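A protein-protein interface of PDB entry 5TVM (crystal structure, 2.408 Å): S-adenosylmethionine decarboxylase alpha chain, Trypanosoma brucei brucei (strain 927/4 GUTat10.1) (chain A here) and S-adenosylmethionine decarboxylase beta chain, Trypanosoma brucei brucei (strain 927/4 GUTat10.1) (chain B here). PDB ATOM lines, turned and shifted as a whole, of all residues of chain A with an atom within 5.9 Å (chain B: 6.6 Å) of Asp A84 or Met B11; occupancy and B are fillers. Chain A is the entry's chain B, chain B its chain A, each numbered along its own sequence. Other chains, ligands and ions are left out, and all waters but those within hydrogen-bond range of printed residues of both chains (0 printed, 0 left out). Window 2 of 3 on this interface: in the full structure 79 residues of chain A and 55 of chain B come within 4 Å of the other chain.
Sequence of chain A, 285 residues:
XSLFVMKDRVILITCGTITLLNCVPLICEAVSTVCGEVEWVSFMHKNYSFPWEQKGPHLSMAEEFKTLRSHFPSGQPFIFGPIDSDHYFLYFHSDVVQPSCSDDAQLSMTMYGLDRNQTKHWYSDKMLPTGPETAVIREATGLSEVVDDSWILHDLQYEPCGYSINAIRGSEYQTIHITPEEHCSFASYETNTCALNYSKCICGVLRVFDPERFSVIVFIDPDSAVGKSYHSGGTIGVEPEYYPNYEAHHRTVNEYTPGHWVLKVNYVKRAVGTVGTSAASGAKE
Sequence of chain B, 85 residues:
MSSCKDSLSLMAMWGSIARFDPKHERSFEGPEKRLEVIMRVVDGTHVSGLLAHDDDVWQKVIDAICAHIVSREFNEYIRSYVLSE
Ile A83 touches Leu B8.
CB of Met B11 touches CG2 of Ile A83, at 3.9 Å.
Ala B12 touches Ile A83.
Asp A84 touches Met B11 (CB to O, 3.4 Å).
Gly B15 touches Asp A84.
His A87 touches Ala B12.
Of the printed residues of chain B, Ile A83 touches Leu B8 (3.5 Å), Met B11 (3.9 Å) and Ala B12 (3.3 Å).
Of chain B, only Met B11 (3.4 Å) and Gly B15 (3.2 Å) come within 4 Å of Asp A84.
Printed residues of chain B within 4 Å of Ser A85: Arg B19 (2.5 Å).
Of the printed residues of chain B, His A87 touches Ala B12.
Asp B6 touches none of the printed residues of chain A.
Leu B10 touches none of the printed residues of chain A.
Of the printed residues of chain A, Met B11 touches Ile A83 and Asp A84.
Of the printed residues of chain A, Ala B12 touches Ile A83 (3.3 Å) and His A87 (3.9 Å).
Printed residues of chain A within 4 Å of Arg B19: Ser A85 (2.5 Å) and Asp A86 (2.8 Å).
The nearest residue of chain A that does not touch Met B11 is Ser A85 (5.6 Å).
The nearest printed residue of chain B that does not touch Ile A83 is Ser B9 (5.5 Å).
The backbone NH (N) of Leu B8 lies within hydrogen-bond range of the side-chain carboxylate (OD1) of Asp B6 (2.9 Å).
O of Ala B12 lies within hydrogen-bond range of OG of Ser B16 (3.3 Å).
A ring nitrogen (ND1) of His A87 is in hydrogen-bond range of the backbone carbonyl oxygen (O) of Pro A82 (3.1 Å).
The backbone carbonyl oxygen (O) of Ile A83 sits close to a ring nitrogen (ND1) of His A87, at 3.0 Å.
The side-chain carboxylate (OD1) of Asp A86 lies within hydrogen-bond range of the side-chain hydroxyl (OG) of Ser A85.
The backbone carbonyl oxygen of Ser A85 lies within hydrogen-bond range of a ring nitrogen (ND1) of His A87 (3.0 Å).
Of the 6 printed residues of chain A, 5 touch a printed residue of chain B.
Along chain A the printed residues that touch a printed residue of chain B span positions 83 to 87.
Among the printed residues, Asp or Glu carboxylates within 4 Å of a Lys or Arg side-chain nitrogen of the other chain: Asp A86 with Arg B19 (2.8 Å).
NH1 of Arg B19 lies within hydrogen-bond range of OG of Ser A85.
The side-chain carboxylate (OD1) of Asp A86 lies within salt-bridge range of the guanidinium group (NH2) of Arg B19 (2.8 Å).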
ATOM      1  N   PRO A  82      -2.917   4.400 -29.341  1.00  0.00           N
ATOM      2  CA  PRO A  82      -2.097   3.761 -28.302  1.00  0.00           C
ATOM      3  C   PRO A  82      -1.204   2.679 -28.888  1.00  0.00           C
ATOM      4  O   PRO A  82      -1.671   1.763 -29.570  1.00  0.00           O
ATOM      5  CB  PRO A  82      -3.137   3.183 -27.336  1.00  0.00           C
ATOM      6  CG  PRO A  82      -4.371   3.020 -28.162  1.00  0.00           C
ATOM      7  CD  PRO A  82      -4.355   4.156 -29.137  1.00  0.00           C
ATOM      8  N   ILE A  83       0.095   2.784 -28.598  1.00  0.00           N
ATOM      9  CA  ILE A  83       1.071   1.905 -29.235  1.00  0.00           C
ATOM     10  C   ILE A  83       0.934   0.478 -28.722  1.00  0.00           C
ATOM     11  O   ILE A  83       1.139  -0.479 -29.478  1.00  0.00           O
ATOM     12  CB  ILE A  83       2.494   2.456 -29.022  1.00  0.00           C
ATOM     13  CG1 ILE A  83       2.578   3.907 -29.514  1.00  0.00           C
ATOM     14  CG2 ILE A  83       3.512   1.583 -29.757  1.00  0.00           C
ATOM     15  CD1 ILE A  83       3.848   4.619 -29.124  1.00  0.00           C
ATOM     16  N   ASP A  84       0.588   0.300 -27.446  1.00  0.00           N
ATOM     17  CA  ASP A  84       0.344  -1.025 -26.893  1.00  0.00           C
ATOM     18  C   ASP A  84      -1.125  -1.430 -26.975  1.00  0.00           C
ATOM     19  O   ASP A  84      -1.562  -2.301 -26.215  1.00  0.00           O
ATOM     20  CB  ASP A  84       0.835  -1.100 -25.442  1.00  0.00           C
ATOM     21  CG  ASP A  84       0.093  -0.156 -24.517  1.00  0.00           C
ATOM     22  OD1 ASP A  84      -0.930   0.428 -24.936  1.00  0.00           O
ATOM     23  OD2 ASP A  84       0.536  -0.002 -23.358  1.00  0.00           O
ATOM     24  N   SER A  85      -1.889  -0.815 -27.869  1.00  0.00           N
ATOM     25  CA  SER A  85      -3.262  -1.226 -28.140  1.00  0.00           C
ATOM     26  C   SER A  85      -3.554  -0.916 -29.607  1.00  0.00           C
ATOM     27  O   SER A  85      -2.636  -0.819 -30.426  1.00  0.00           O
ATOM     28  CB  SER A  85      -4.231  -0.537 -27.163  1.00  0.00           C
ATOM     29  OG  SER A  85      -5.568  -0.941 -27.406  1.00  0.00           O
ATOM     30  N   ASP A  86      -4.834  -0.753 -29.941  1.00  0.00           N
ATOM     31  CA  ASP A  86      -5.231  -0.528 -31.325  1.00  0.00           C
ATOM     32  C   ASP A  86      -4.601   0.752 -31.864  1.00  0.00           C
ATOM     33  O   ASP A  86      -4.876   1.847 -31.363  1.00  0.00           O
ATOM     34  CB  ASP A  86      -6.756  -0.454 -31.423  1.00  0.00           C
ATOM     35  CG  ASP A  86      -7.433  -1.743 -30.990  1.00  0.00           C
ATOM     36  OD1 ASP A  86      -7.567  -1.961 -29.769  1.00  0.00           O
ATOM     37  OD2 ASP A  86      -7.833  -2.536 -31.869  1.00  0.00           O
ATOM     38  N   HIS A  87      -3.758   0.615 -32.887  1.00  0.00           N
ATOM     39  CA  HIS A  87      -3.145   1.768 -33.530  1.00  0.00           C
ATOM     40  C   HIS A  87      -2.850   1.435 -34.987  1.00  0.00           C
ATOM     41  O   HIS A  87      -2.930   0.280 -35.415  1.00  0.00           O
ATOM     42  CB  HIS A  87      -1.866   2.207 -32.805  1.00  0.00           C
ATOM     43  CG  HIS A  87      -0.718   1.261 -32.973  1.00  0.00           C
ATOM     44  ND1 HIS A  87      -0.335   0.372 -31.992  1.00  0.00           N
ATOM     45  CD2 HIS A  87       0.143   1.076 -34.003  1.00  0.00           C
ATOM     46  CE1 HIS A  87       0.705  -0.324 -32.411  1.00  0.00           C
ATOM     47  NE2 HIS A  87       1.015   0.082 -33.629  1.00  0.00           N
ATOM     48  N   ASP B   6      13.091  -2.628 -31.434  1.00  0.00           N
ATOM     49  CA  ASP B   6      12.923  -1.243 -31.023  1.00  0.00           C
ATOM     50  C   ASP B   6      11.862  -1.130 -29.930  1.00  0.00           C
ATOM     51  O   ASP B   6      11.002  -2.000 -29.766  1.00  0.00           O
ATOM     52  CB  ASP B   6      12.546  -0.367 -32.220  1.00  0.00           C
ATOM     53  CG  ASP B   6      11.130  -0.612 -32.703  1.00  0.00           C
ATOM     54  OD1 ASP B   6      10.208   0.051 -32.184  1.00  0.00           O
ATOM     55  OD2 ASP B   6      10.939  -1.458 -33.604  1.00  0.00           O
ATOM     56  N   SER B   7      11.933  -0.032 -29.176  1.00  0.00           N
ATOM     57  CA  SER B   7      11.041   0.140 -28.034  1.00  0.00           C
ATOM     58  C   SER B   7       9.582   0.210 -28.469  1.00  0.00           C
ATOM     59  O   SER B   7       8.701  -0.347 -27.804  1.00  0.00           O
ATOM     60  CB  SER B   7      11.431   1.394 -27.250  1.00  0.00           C
ATOM     61  OG  SER B   7      11.385   2.547 -28.071  1.00  0.00           O
ATOM     62  N   LEU B   8       9.303   0.891 -29.583  1.00  0.00           N
ATOM     63  CA  LEU B   8       7.920   1.050 -30.024  1.00  0.00           C
ATOM     64  C   LEU B   8       7.311  -0.292 -30.412  1.00  0.00           C
ATOM     65  O   LEU B   8       6.183  -0.611 -30.015  1.00  0.00           O
ATOM     66  CB  LEU B   8       7.852   2.033 -31.191  1.00  0.00           C
ATOM     67  CG  LEU B   8       8.413   3.427 -30.904  1.00  0.00           C
ATOM     68  CD1 LEU B   8       8.286   4.310 -32.136  1.00  0.00           C
ATOM     69  CD2 LEU B   8       7.719   4.070 -29.708  1.00  0.00           C
ATOM     70  N   SER B   9       8.039  -1.093 -31.190  1.00  0.00           N
ATOM     71  CA  SER B   9       7.546  -2.421 -31.537  1.00  0.00           C
ATOM     72  C   SER B   9       7.482  -3.325 -30.314  1.00  0.00           C
ATOM     73  O   SER B   9       6.665  -4.250 -30.271  1.00  0.00           O
ATOM     74  CB  SER B   9       8.429  -3.042 -32.616  1.00  0.00           C
ATOM     75  OG  SER B   9       8.370  -2.281 -33.809  1.00  0.00           O
ATOM     76  N   LEU B  10       8.331  -3.076 -29.317  1.00  0.00           N
ATOM     77  CA  LEU B  10       8.245  -3.819 -28.066  1.00  0.00           C
ATOM     78  C   LEU B  10       6.936  -3.518 -27.345  1.00  0.00           C
ATOM     79  O   LEU B  10       6.287  -4.428 -26.816  1.00  0.00           O
ATOM     80  CB  LEU B  10       9.447  -3.482 -27.184  1.00  0.00           C
ATOM     81  CG  LEU B  10       9.680  -4.304 -25.914  1.00  0.00           C
ATOM     82  CD1 LEU B  10      11.147  -4.223 -25.523  1.00  0.00           C
ATOM     83  CD2 LEU B  10       8.804  -3.831 -24.754  1.00  0.00           C
ATOM     84  N   MET B  11       6.534  -2.243 -27.312  1.00  0.00           N
ATOM     85  CA  MET B  11       5.243  -1.887 -26.732  1.00  0.00           C
ATOM     86  C   MET B  11       4.102  -2.527 -27.508  1.00  0.00           C
ATOM     87  O   MET B  11       3.151  -3.049 -26.915  1.00  0.00           O
ATOM     88  CB  MET B  11       5.071  -0.369 -26.712  1.00  0.00           C
ATOM     89  CG  MET B  11       6.126   0.369 -25.924  1.00  0.00           C
ATOM     90  SD  MET B  11       6.129   2.125 -26.303  1.00  0.00           S
ATOM     91  CE  MET B  11       7.837   2.529 -25.939  1.00  0.00           C
ATOM     92  N   ALA B  12       4.174  -2.486 -28.840  1.00  0.00           N
ATOM     93  CA  ALA B  12       3.126  -3.088 -29.655  1.00  0.00           C
ATOM     94  C   ALA B  12       2.985  -4.572 -29.353  1.00  0.00           C
ATOM     95  O   ALA B  12       1.867  -5.097 -29.286  1.00  0.00           O
ATOM     96  CB  ALA B  12       3.424  -2.871 -31.138  1.00  0.00           C
ATOM     97  N   MET B  13       4.108  -5.265 -29.154  1.00  0.00           N
ATOM     98  CA  MET B  13       4.044  -6.699 -28.899  1.00  0.00           C
ATOM     99  C   MET B  13       3.387  -6.993 -27.557  1.00  0.00           C
ATOM    100  O   MET B  13       2.573  -7.918 -27.450  1.00  0.00           O
ATOM    101  CB  MET B  13       5.444  -7.308 -28.950  1.00  0.00           C
ATOM    102  CG  MET B  13       5.434  -8.827 -29.044  1.00  0.00           C
ATOM    103  SD  MET B  13       7.068  -9.565 -28.913  1.00  0.00           S
ATOM    104  CE  MET B  13       7.938  -8.709 -30.223  1.00  0.00           C
ATOM    105  N   TRP B  14       3.725  -6.220 -26.521  1.00  0.00           N
ATOM    106  CA  TRP B  14       3.116  -6.446 -25.214  1.00  0.00           C
ATOM    107  C   TRP B  14       1.606  -6.270 -25.263  1.00  0.00           C
ATOM    108  O   TRP B  14       0.876  -6.960 -24.542  1.00  0.00           O
ATOM    109  CB  TRP B  14       3.717  -5.506 -24.172  1.00  0.00           C
ATOM    110  CG  TRP B  14       3.166  -5.744 -22.800  1.00  0.00           C
ATOM    111  CD1 TRP B  14       2.362  -4.909 -22.081  1.00  0.00           C
ATOM    112  CD2 TRP B  14       3.367  -6.906 -21.986  1.00  0.00           C
ATOM    113  NE1 TRP B  14       2.056  -5.474 -20.867  1.00  0.00           N
ATOM    114  CE2 TRP B  14       2.659  -6.703 -20.785  1.00  0.00           C
ATOM    115  CE3 TRP B  14       4.078  -8.099 -22.157  1.00  0.00           C
ATOM    116  CZ2 TRP B  14       2.645  -7.644 -19.757  1.00  0.00           C
ATOM    117  CZ3 TRP B  14       4.061  -9.033 -21.136  1.00  0.00           C
ATOM    118  CH2 TRP B  14       3.350  -8.801 -19.952  1.00  0.00           C
ATOM    119  N   GLY B  15       1.118  -5.351 -26.100  1.00  0.00           N
ATOM    120  CA  GLY B  15      -0.316  -5.199 -26.262  1.00  0.00           C
ATOM    121  C   GLY B  15      -0.956  -6.374 -26.969  1.00  0.00           C
ATOM    122  O   GLY B  15      -2.110  -6.715 -26.695  1.00  0.00           O
ATOM    123  N   SER B  16      -0.222  -7.010 -27.884  1.00  0.00           N
ATOM    124  CA  SER B  16      -0.741  -8.179 -28.583  1.00  0.00           C
ATOM    125  C   SER B  16      -0.677  -9.429 -27.716  1.00  0.00           C
ATOM    126  O   SER B  16      -1.528 -10.316 -27.850  1.00  0.00           O
ATOM    127  CB  SER B  16       0.039  -8.409 -29.879  1.00  0.00           C
ATOM    128  OG  SER B  16      -0.093  -7.309 -30.761  1.00  0.00           O
ATOM    129  N   ARG B  19      -3.606  -9.752 -25.195  1.00  0.00           N
ATOM    130  CA  ARG B  19      -4.851 -10.155 -25.835  1.00  0.00           C
ATOM    131  C   ARG B  19      -4.721 -11.489 -26.562  1.00  0.00           C
ATOM    132  O   ARG B  19      -5.542 -11.795 -27.434  1.00  0.00           O
ATOM    133  CB  ARG B  19      -5.312  -9.072 -26.812  1.00  0.00           C
ATOM    134  CG  ARG B  19      -5.551  -7.719 -26.167  1.00  0.00           C
ATOM    135  CD  ARG B  19      -5.875  -6.654 -27.200  1.00  0.00           C
ATOM    136  NE  ARG B  19      -6.052  -5.344 -26.583  1.00  0.00           N
ATOM    137  CZ  ARG B  19      -6.345  -4.231 -27.250  1.00  0.00           C
ATOM    138  NH1 ARG B  19      -6.485  -3.087 -26.596  1.00  0.00           N
ATOM    139  NH2 ARG B  19      -6.496  -4.257 -28.568  1.00  0.00           N
